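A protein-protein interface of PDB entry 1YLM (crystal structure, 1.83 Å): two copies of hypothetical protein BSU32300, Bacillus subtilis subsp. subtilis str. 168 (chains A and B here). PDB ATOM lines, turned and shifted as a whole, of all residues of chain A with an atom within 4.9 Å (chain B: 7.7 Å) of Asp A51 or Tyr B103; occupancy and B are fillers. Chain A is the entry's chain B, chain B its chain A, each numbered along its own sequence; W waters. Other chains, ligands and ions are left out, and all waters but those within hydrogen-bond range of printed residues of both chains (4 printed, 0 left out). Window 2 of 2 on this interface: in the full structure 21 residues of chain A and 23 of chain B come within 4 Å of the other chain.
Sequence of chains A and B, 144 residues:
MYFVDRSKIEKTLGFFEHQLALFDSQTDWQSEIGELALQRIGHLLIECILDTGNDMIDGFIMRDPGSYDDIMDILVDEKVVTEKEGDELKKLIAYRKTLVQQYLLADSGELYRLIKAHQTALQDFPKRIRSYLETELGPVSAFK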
ATOM      1  N   LYS A   8      16.566  34.965 -23.485  1.00  0.00           N
ATOM      2  CA  LYS A   8      17.492  33.976 -22.904  1.00  0.00           C
ATOM      3  C   LYS A   8      18.932  34.510 -22.976  1.00  0.00           C
ATOM      4  O   LYS A   8      19.646  34.488 -21.974  1.00  0.00           O
ATOM      5  CB  LYS A   8      17.356  32.641 -23.608  1.00  0.00           C
ATOM      6  CG  LYS A   8      18.280  31.499 -23.087  1.00  0.00           C
ATOM      7  CD  LYS A   8      17.920  30.200 -23.811  1.00  0.00           C
ATOM      8  CE  LYS A   8      18.679  28.998 -23.245  1.00  0.00           C
ATOM      9  NZ  LYS A   8      20.100  29.001 -23.731  1.00  0.00           N
ATOM     10  N   THR A  12      21.184  35.561 -19.811  1.00  0.00           N
ATOM     11  CA  THR A  12      22.423  34.779 -19.655  1.00  0.00           C
ATOM     12  C   THR A  12      23.640  35.719 -19.548  1.00  0.00           C
ATOM     13  O   THR A  12      24.531  35.485 -18.742  1.00  0.00           O
ATOM     14  CB  THR A  12      22.567  33.728 -20.767  1.00  0.00           C
ATOM     15  OG1 THR A  12      21.480  32.805 -20.660  1.00  0.00           O
ATOM     16  CG2 THR A  12      23.889  32.924 -20.631  1.00  0.00           C
ATOM     17  N   PHE A  15      23.745  37.260 -16.004  1.00  0.00           N
ATOM     18  CA  PHE A  15      24.246  36.258 -15.053  1.00  0.00           C
ATOM     19  C   PHE A  15      25.767  36.130 -15.201  1.00  0.00           C
ATOM     20  O   PHE A  15      26.495  36.116 -14.221  1.00  0.00           O
ATOM     21  CB  PHE A  15      23.543  34.934 -15.345  1.00  0.00           C
ATOM     22  CG  PHE A  15      23.917  33.800 -14.422  1.00  0.00           C
ATOM     23  CD1 PHE A  15      23.219  33.588 -13.236  1.00  0.00           C
ATOM     24  CD2 PHE A  15      24.928  32.897 -14.780  1.00  0.00           C
ATOM     25  CE1 PHE A  15      23.536  32.507 -12.403  1.00  0.00           C
ATOM     26  CE2 PHE A  15      25.253  31.830 -13.962  1.00  0.00           C
ATOM     27  CZ  PHE A  15      24.559  31.635 -12.766  1.00  0.00           C
ATOM     28  N   ARG A  40      33.296  26.815  -9.697  1.00  0.00           N
ATOM     29  CA  ARG A  40      31.906  27.069 -10.104  1.00  0.00           C
ATOM     30  C   ARG A  40      31.863  28.275 -11.045  1.00  0.00           C
ATOM     31  O   ARG A  40      31.217  28.237 -12.107  1.00  0.00           O
ATOM     32  CB  ARG A  40      30.992  27.293  -8.888  1.00  0.00           C
ATOM     33  CG  ARG A  40      29.483  27.434  -9.274  1.00  0.00           C
ATOM     34  CD  ARG A  40      28.934  26.154  -9.878  1.00  0.00           C
ATOM     35  NE  ARG A  40      27.518  26.292 -10.239  1.00  0.00           N
ATOM     36  CZ  ARG A  40      26.855  25.443 -11.025  1.00  0.00           C
ATOM     37  NH1 ARG A  40      27.467  24.368 -11.532  1.00  0.00           N
ATOM     38  NH2 ARG A  40      25.568  25.675 -11.311  1.00  0.00           N
ATOM     39  N   LEU A  44      30.565  28.215 -14.851  1.00  0.00           N
ATOM     40  CA  LEU A  44      29.487  29.139 -15.244  1.00  0.00           C
ATOM     41  C   LEU A  44      29.886  30.061 -16.403  1.00  0.00           C
ATOM     42  O   LEU A  44      29.092  30.280 -17.317  1.00  0.00           O
ATOM     43  CB  LEU A  44      29.003  29.975 -14.060  1.00  0.00           C
ATOM     44  CG  LEU A  44      28.286  29.137 -12.986  1.00  0.00           C
ATOM     45  CD1 LEU A  44      27.894  30.009 -11.809  1.00  0.00           C
ATOM     46  CD2 LEU A  44      27.057  28.424 -13.587  1.00  0.00           C
ATOM     47  N   GLU A  47      29.958  27.977 -19.593  1.00  0.00           N
ATOM     48  CA  GLU A  47      28.627  27.568 -20.059  1.00  0.00           C
ATOM     49  C   GLU A  47      27.841  28.742 -20.628  1.00  0.00           C
ATOM     50  O   GLU A  47      27.175  28.593 -21.657  1.00  0.00           O
ATOM     51  CB  GLU A  47      27.804  26.895 -18.961  1.00  0.00           C
ATOM     52  CG  GLU A  47      28.280  25.519 -18.501  1.00  0.00           C
ATOM     53  CD  GLU A  47      28.686  24.590 -19.645  1.00  0.00           C
ATOM     54  OE1 GLU A  47      27.817  23.977 -20.316  1.00  0.00           O
ATOM     55  OE2 GLU A  47      29.896  24.486 -19.878  1.00  0.00           O
ATOM     56  N   CYS A  48      27.942  29.908 -19.985  1.00  0.00           N
ATOM     57  CA  CYS A  48      27.303  31.126 -20.507  1.00  0.00           C
ATOM     58  C   CYS A  48      27.774  31.465 -21.919  1.00  0.00           C
ATOM     59  O   CYS A  48      26.970  31.857 -22.766  1.00  0.00           O
ATOM     60  CB  CYS A  48      27.546  32.331 -19.587  1.00  0.00           C
ATOM     61  SG  CYS A  48      26.629  32.259 -17.997  1.00  0.00           S
ATOM     62  N   ILE A  49      29.077  31.342 -22.163  1.00  0.00           N
ATOM     63  CA  ILE A  49      29.634  31.626 -23.483  1.00  0.00           C
ATOM     64  C   ILE A  49      29.115  30.632 -24.522  1.00  0.00           C
ATOM     65  O   ILE A  49      28.667  31.035 -25.593  1.00  0.00           O
ATOM     66  CB  ILE A  49      31.182  31.631 -23.462  1.00  0.00           C
ATOM     67  CG1 ILE A  49      31.694  32.862 -22.712  1.00  0.00           C
ATOM     68  CG2 ILE A  49      31.761  31.566 -24.886  1.00  0.00           C
ATOM     69  CD1 ILE A  49      33.143  32.696 -22.175  1.00  0.00           C
ATOM     70  N   LEU A  50      29.171  29.343 -24.196  1.00  0.00           N
ATOM     71  CA  LEU A  50      28.753  28.300 -25.148  1.00  0.00           C
ATOM     72  C   LEU A  50      27.247  28.383 -25.455  1.00  0.00           C
ATOM     73  O   LEU A  50      26.828  28.300 -26.610  1.00  0.00           O
ATOM     74  CB  LEU A  50      29.133  26.923 -24.607  1.00  0.00           C
ATOM     75  CG  LEU A  50      30.641  26.709 -24.414  1.00  0.00           C
ATOM     76  CD1 LEU A  50      30.899  25.337 -23.779  1.00  0.00           C
ATOM     77  CD2 LEU A  50      31.421  26.898 -25.724  1.00  0.00           C
ATOM     78  N   ASP A  51      26.443  28.565 -24.414  1.00  0.00           N
ATOM     79  CA  ASP A  51      24.986  28.638 -24.582  1.00  0.00           C
ATOM     80  C   ASP A  51      24.601  29.871 -25.388  1.00  0.00           C
ATOM     81  O   ASP A  51      23.791  29.775 -26.312  1.00  0.00           O
ATOM     82  CB  ASP A  51      24.280  28.642 -23.219  1.00  0.00           C
ATOM     83  CG  ASP A  51      24.298  27.268 -22.545  1.00  0.00           C
ATOM     84  OD1 ASP A  51      24.479  26.250 -23.248  1.00  0.00           O
ATOM     85  OD2 ASP A  51      24.135  27.224 -21.312  1.00  0.00           O
ATOM     86  N   THR A  52      25.193  31.019 -25.053  1.00  0.00           N
ATOM     87  CA  THR A  52      24.930  32.257 -25.807  1.00  0.00           C
ATOM     88  C   THR A  52      25.389  32.071 -27.271  1.00  0.00           C
ATOM     89  O   THR A  52      24.658  32.406 -28.195  1.00  0.00           O
ATOM     90  CB  THR A  52      25.606  33.483 -25.152  1.00  0.00           C
ATOM     91  OG1 THR A  52      25.064  33.687 -23.830  1.00  0.00           O
ATOM     92  CG2 THR A  52      25.379  34.757 -25.998  1.00  0.00           C
ATOM     93  N   GLY A  53      26.584  31.517 -27.465  1.00  0.00           N
ATOM     94  CA  GLY A  53      27.075  31.154 -28.800  1.00  0.00           C
ATOM     95  C   GLY A  53      26.085  30.296 -29.577  1.00  0.00           C
ATOM     96  O   GLY A  53      25.691  30.657 -30.693  1.00  0.00           O
ATOM     97  N   ASN A  54      25.669  29.180 -28.985  1.00  0.00           N
ATOM     98  CA  ASN A  54      24.622  28.326 -29.560  1.00  0.00           C
ATOM     99  C   ASN A  54      23.329  29.072 -29.885  1.00  0.00           C
ATOM    100  O   ASN A  54      22.751  28.860 -30.951  1.00  0.00           O
ATOM    101  CB  ASN A  54      24.322  27.135 -28.650  1.00  0.00           C
ATOM    102  CG  ASN A  54      25.263  25.961 -28.883  1.00  0.00           C
ATOM    103  OD1 ASN A  54      25.598  25.221 -27.945  1.00  0.00           O
ATOM    104  ND2 ASN A  54      25.678  25.763 -30.130  1.00  0.00           N
ATOM    105  N   ASP A  55      22.865  29.936 -28.977  1.00  0.00           N
ATOM    106  CA  ASP A  55      21.630  30.717 -29.233  1.00  0.00           C
ATOM    107  C   ASP A  55      21.805  31.718 -30.381  1.00  0.00           C
ATOM    108  O   ASP A  55      20.906  31.891 -31.222  1.00  0.00           O
ATOM    109  CB  ASP A  55      21.140  31.437 -27.960  1.00  0.00           C
ATOM    110  CG  ASP A  55      20.629  30.475 -26.890  1.00  0.00           C
ATOM    111  OD1 ASP A  55      20.149  29.368 -27.229  1.00  0.00           O
ATOM    112  OD2 ASP A  55      20.716  30.830 -25.690  1.00  0.00           O
ATOM    113  N   GLN B  39      27.260  25.097  -4.656  1.00  0.00           N
ATOM    114  CA  GLN B  39      26.888  24.557  -5.996  1.00  0.00           C
ATOM    115  C   GLN B  39      27.954  23.601  -6.552  1.00  0.00           C
ATOM    116  O   GLN B  39      27.628  22.538  -7.104  1.00  0.00           O
ATOM    117  CB  GLN B  39      26.600  25.685  -6.999  1.00  0.00           C
ATOM    118  CG  GLN B  39      25.312  26.476  -6.667  1.00  0.00           C
ATOM    119  CD  GLN B  39      25.183  27.748  -7.476  1.00  0.00           C
ATOM    120  OE1 GLN B  39      25.869  27.930  -8.478  1.00  0.00           O
ATOM    121  NE2 GLN B  39      24.284  28.623  -7.057  1.00  0.00           N
ATOM    122  N   ARG B  96      20.873  17.511 -10.656  1.00  0.00           N
ATOM    123  CA  ARG B  96      21.964  17.631 -11.617  1.00  0.00           C
ATOM    124  C   ARG B  96      21.628  18.568 -12.768  1.00  0.00           C
ATOM    125  O   ARG B  96      22.432  19.412 -13.118  1.00  0.00           O
ATOM    126  CB  ARG B  96      22.379  16.269 -12.175  1.00  0.00           C
ATOM    127  CG  ARG B  96      23.707  16.317 -12.937  1.00  0.00           C
ATOM    128  CD  ARG B  96      23.996  14.981 -13.628  1.00  0.00           C
ATOM    129  NE  ARG B  96      25.293  15.000 -14.309  1.00  0.00           N
ATOM    130  CZ  ARG B  96      25.485  15.277 -15.596  1.00  0.00           C
ATOM    131  NH1 ARG B  96      24.461  15.561 -16.406  1.00  0.00           N
ATOM    132  NH2 ARG B  96      26.720  15.262 -16.087  1.00  0.00           N
ATOM    133  N   LYS B  97      20.446  18.416 -13.359  1.00  0.00           N
ATOM    134  CA  LYS B  97      20.091  19.232 -14.526  1.00  0.00           C
ATOM    135  C   LYS B  97      20.103  20.729 -14.196  1.00  0.00           C
ATOM    136  O   LYS B  97      20.557  21.540 -15.002  1.00  0.00           O
ATOM    137  CB  LYS B  97      18.722  18.815 -15.095  1.00  0.00           C
ATOM    138  CG  LYS B  97      18.320  19.539 -16.376  1.00  0.00           C
ATOM    139  CD  LYS B  97      16.903  19.113 -16.807  1.00  0.00           C
ATOM    140  CE  LYS B  97      16.516  19.679 -18.188  1.00  0.00           C
ATOM    141  NZ  LYS B  97      15.166  19.145 -18.639  1.00  0.00           N
ATOM    142  N   THR B  98      19.623  21.083 -13.007  1.00  0.00           N
ATOM    143  CA  THR B  98      19.670  22.470 -12.549  1.00  0.00           C
ATOM    144  C   THR B  98      21.109  22.975 -12.437  1.00  0.00           C
ATOM    145  O   THR B  98      21.425  24.093 -12.861  1.00  0.00           O
ATOM    146  CB  THR B  98      18.928  22.649 -11.206  1.00  0.00           C
ATOM    147  OG1 THR B  98      17.551  22.264 -11.381  1.00  0.00           O
ATOM    148  CG2 THR B  98      18.989  24.108 -10.761  1.00  0.00           C
ATOM    149  N   LEU B  99      21.984  22.142 -11.884  1.00  0.00           N
ATOM    150  CA  LEU B  99      23.383  22.540 -11.688  1.00  0.00           C
ATOM    151  C   LEU B  99      24.182  22.661 -12.977  1.00  0.00           C
ATOM    152  O   LEU B  99      25.021  23.562 -13.094  1.00  0.00           O
ATOM    153  CB  LEU B  99      24.075  21.585 -10.712  1.00  0.00           C
ATOM    154  CG  LEU B  99      23.683  21.804  -9.248  1.00  0.00           C
ATOM    155  CD1 LEU B  99      24.111  20.589  -8.420  1.00  0.00           C
ATOM    156  CD2 LEU B  99      24.306  23.093  -8.683  1.00  0.00           C
ATOM    157  N   VAL B 100      23.920  21.775 -13.946  1.00  0.00           N
ATOM    158  CA  VAL B 100      24.763  21.695 -15.153  1.00  0.00           C
ATOM    159  C   VAL B 100      24.150  22.304 -16.415  1.00  0.00           C
ATOM    160  O   VAL B 100      24.876  22.706 -17.327  1.00  0.00           O
ATOM    161  CB  VAL B 100      25.238  20.246 -15.448  1.00  0.00           C
ATOM    162  CG1 VAL B 100      25.855  19.629 -14.189  1.00  0.00           C
ATOM    163  CG2 VAL B 100      24.105  19.398 -15.977  1.00  0.00           C
ATOM    164  N   GLN B 101      22.826  22.348 -16.472  1.00  0.00           N
ATOM    165  CA  GLN B 101      22.131  22.796 -17.670  1.00  0.00           C
ATOM    166  C   GLN B 101      21.280  24.049 -17.432  1.00  0.00           C
ATOM    167  O   GLN B 101      21.350  24.994 -18.216  1.00  0.00           O
ATOM    168  CB  GLN B 101      21.278  21.655 -18.220  1.00  0.00           C
ATOM    169  CG  GLN B 101      20.658  21.938 -19.569  1.00  0.00           C
ATOM    170  CD  GLN B 101      19.734  20.820 -20.005  1.00  0.00           C
ATOM    171  OE1 GLN B 101      20.061  19.641 -19.858  1.00  0.00           O
ATOM    172  NE2 GLN B 101      18.567  21.181 -20.535  1.00  0.00           N
ATOM    173  N   GLN B 102      20.492  24.056 -16.361  1.00  0.00           N
ATOM    174  CA  GLN B 102      19.602  25.184 -16.070  1.00  0.00           C
ATOM    175  C   GLN B 102      20.151  25.990 -14.895  1.00  0.00           C
ATOM    176  O   GLN B 102      19.466  26.253 -13.897  1.00  0.00           O
ATOM    177  CB  GLN B 102      18.162  24.697 -15.813  1.00  0.00           C
ATOM    178  CG  GLN B 102      17.497  24.013 -17.031  1.00  0.00           C
ATOM    179  CD  GLN B 102      16.185  23.304 -16.678  1.00  0.00           C
ATOM    180  OE1 GLN B 102      15.943  22.942 -15.528  1.00  0.00           O
ATOM    181  NE2 GLN B 102      15.346  23.083 -17.684  1.00  0.00           N
ATOM    182  N   TYR B 103      21.403  26.405 -15.040  1.00  0.00           N
ATOM    183  CA  TYR B 103      22.158  26.976 -13.936  1.00  0.00           C
ATOM    184  C   TYR B 103      21.663  28.363 -13.514  1.00  0.00           C
ATOM    185  O   TYR B 103      21.934  28.785 -12.391  1.00  0.00           O
ATOM    186  CB  TYR B 103      23.655  26.994 -14.265  1.00  0.00           C
ATOM    187  CG  TYR B 103      23.952  27.560 -15.631  1.00  0.00           C
ATOM    188  CD1 TYR B 103      24.033  28.949 -15.837  1.00  0.00           C
ATOM    189  CD2 TYR B 103      24.143  26.711 -16.723  1.00  0.00           C
ATOM    190  CE1 TYR B 103      24.303  29.472 -17.106  1.00  0.00           C
ATOM    191  CE2 TYR B 103      24.403  27.215 -17.986  1.00  0.00           C
ATOM    192  CZ  TYR B 103      24.486  28.595 -18.169  1.00  0.00           C
ATOM    193  OH  TYR B 103      24.765  29.073 -19.426  1.00  0.00           O
ATOM    194  N   LEU B 104      20.920  29.058 -14.391  1.00  0.00           N
ATOM    195  CA  LEU B 104      20.284  30.323 -13.967  1.00  0.00           C
ATOM    196  C   LEU B 104      19.293  30.098 -12.822  1.00  0.00           C
ATOM    197  O   LEU B 104      18.989  31.020 -12.053  1.00  0.00           O
ATOM    198  CB  LEU B 104      19.573  31.055 -15.113  1.00  0.00           C
ATOM    199  CG  LEU B 104      20.329  31.643 -16.317  1.00  0.00           C
ATOM    200  CD1 LEU B 104      19.629  32.881 -16.862  1.00  0.00           C
ATOM    201  CD2 LEU B 104      21.783  31.957 -16.041  1.00  0.00           C
ATOM    202  N   LEU B 105      18.786  28.872 -12.728  1.00  0.00           N
ATOM    203  CA  LEU B 105      17.769  28.500 -11.735  1.00  0.00           C
ATOM    204  C   LEU B 105      18.340  27.913 -10.432  1.00  0.00           C
ATOM    205  O   LEU B 105      17.592  27.660  -9.475  1.00  0.00           O
ATOM    206  CB  LEU B 105      16.776  27.506 -12.364  1.00  0.00           C
ATOM    207  CG  LEU B 105      16.299  27.850 -13.783  1.00  0.00           C
ATOM    208  CD1 LEU B 105      15.191  26.903 -14.242  1.00  0.00           C
ATOM    209  CD2 LEU B 105      15.855  29.324 -13.851  1.00  0.00           C
ATOM    210  N   ALA B 106      19.655  27.688 -10.387  1.00  0.00           N
ATOM    211  CA  ALA B 106      20.267  27.089  -9.195  1.00  0.00           C
ATOM    212  C   ALA B 106      19.972  27.914  -7.941  1.00  0.00           C
ATOM    213  O   ALA B 106      20.047  29.145  -7.957  1.00  0.00           O
ATOM    214  CB  ALA B 106      21.784  26.886  -9.389  1.00  0.00           C
ATOM    215  N   ASP B 107      19.616  27.223  -6.864  1.00  0.00           N
ATOM    216  CA  ASP B 107      19.204  27.843  -5.604  1.00  0.00           C
ATOM    217  C   ASP B 107      20.008  27.163  -4.504  1.00  0.00           C
ATOM    218  O   ASP B 107      19.714  26.050  -4.114  1.00  0.00           O
ATOM    219  CB  ASP B 107      17.684  27.654  -5.408  1.00  0.00           C
ATOM    220  CG  ASP B 107      17.159  28.172  -4.051  1.00  0.00           C
ATOM    221  OD1 ASP B 107      17.940  28.477  -3.128  1.00  0.00           O
ATOM    222  OD2 ASP B 107      15.912  28.250  -3.912  1.00  0.00           O
HETATM  223  O   HOH W   1      25.279  23.419 -19.937  1.00  0.00           O
HETATM  224  O   HOH W   2      27.728  21.986 -17.846  1.00  0.00           O
HETATM  225  O   HOH W   3      24.438  28.350 -10.961  1.00  0.00           O
HETATM  226  O   HOH W   4      23.035  24.921 -20.648  1.00  0.00           O
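The guanidinium group (NE) of Arg A40 lies within hydrogen-bond range of the side-chain amide oxygen (OE1) of Gln B39 (2.9 Å). The backbone carbonyl oxygen of Leu B99 is in hydrogen-bond range of the guanidinium group of Arg A40 (2.8 Å). The side-chain hydroxyl (OH) of Tyr B103 lies close to the backbone carbonyl oxygen (O) of Glu A47, 3.3 Å away. The side-chain hydroxyl (OH) of Tyr B103 lies within hydrogen-bond range of the backbone NH (N) of Cys A48. The side-chain carboxylate (OD2) of Asp A51 lies within hydrogen-bond range of the side-chain hydroxyl (OH) of Tyr B103 (2.7 Å).
The backbone NH (N) of Tyr B103 lies close to the backbone carbonyl oxygen (O) of Thr B98 (3.2 Å). The backbone carbonyl oxygen (O) of Leu A44 is in hydrogen-bond range of the side-chain sulfur (SG) of Cys A48 (3.2 Å). The backbone carbonyl oxygen (O) of Cys A48 lies within hydrogen-bond range of the side-chain hydroxyl (OG1) of Thr A52, at 2.8 Å.
CD1 of Tyr B103 touches CE2 of Phe A15, 3.6 Å away. Leu B104 touches Phe A15. CB of Tyr B103 touches NH2 of Arg A40, at 3.8 Å. CD2 of Leu A44 touches CB of Tyr B103, 3.8 Å away.
Asp A51 touches one residue of chain B. Tyr B103 touches just these residues of chain A: Phe A15 (3.6 Å), Arg A40 (3.8 Å), Leu A44 (3.8 Å), Glu A47 (3.3 Å), Cys A48 (3.3 Å) and Asp A51 (2.7 Å). Of the printed residues of chain B, Phe A15 touches Tyr B103 and Leu B104. Of the printed residues of chain B, Glu A47 touches Tyr B103 (3.3 Å). Ala B106 touches none of the printed residues of chain A. The nearest printed residue of chain B that does not touch Arg A40 is Ala B106 (4.4 Å).
Of the 14 printed residues of chain A, 6 touch a printed residue of chain B. Printed residues of chain B that touch a printed residue of chain A: Gln B39, Leu B99, Tyr B103 and Leu B104. Among the printed residues, no Asp or Glu carboxylate lies within 4 Å of a Lys or Arg side-chain nitrogen of the other chain.
No position is printed for both chains.
Water W1 bridges OE1 of Glu A47 and O of Val B100. Water W4 lies within hydrogen-bond range of the side-chain carboxylate (OD2) of Asp A51 (2.6 Å) and the backbone carbonyl oxygen (O) of Gln B101 (3.0 Å). Water W3 lies within hydrogen-bond range of OE1 of Gln B39, O of Tyr B103 and NH2 of Arg A40. Water W2 bridges O of Val B100 and OE1 of Glu A47.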
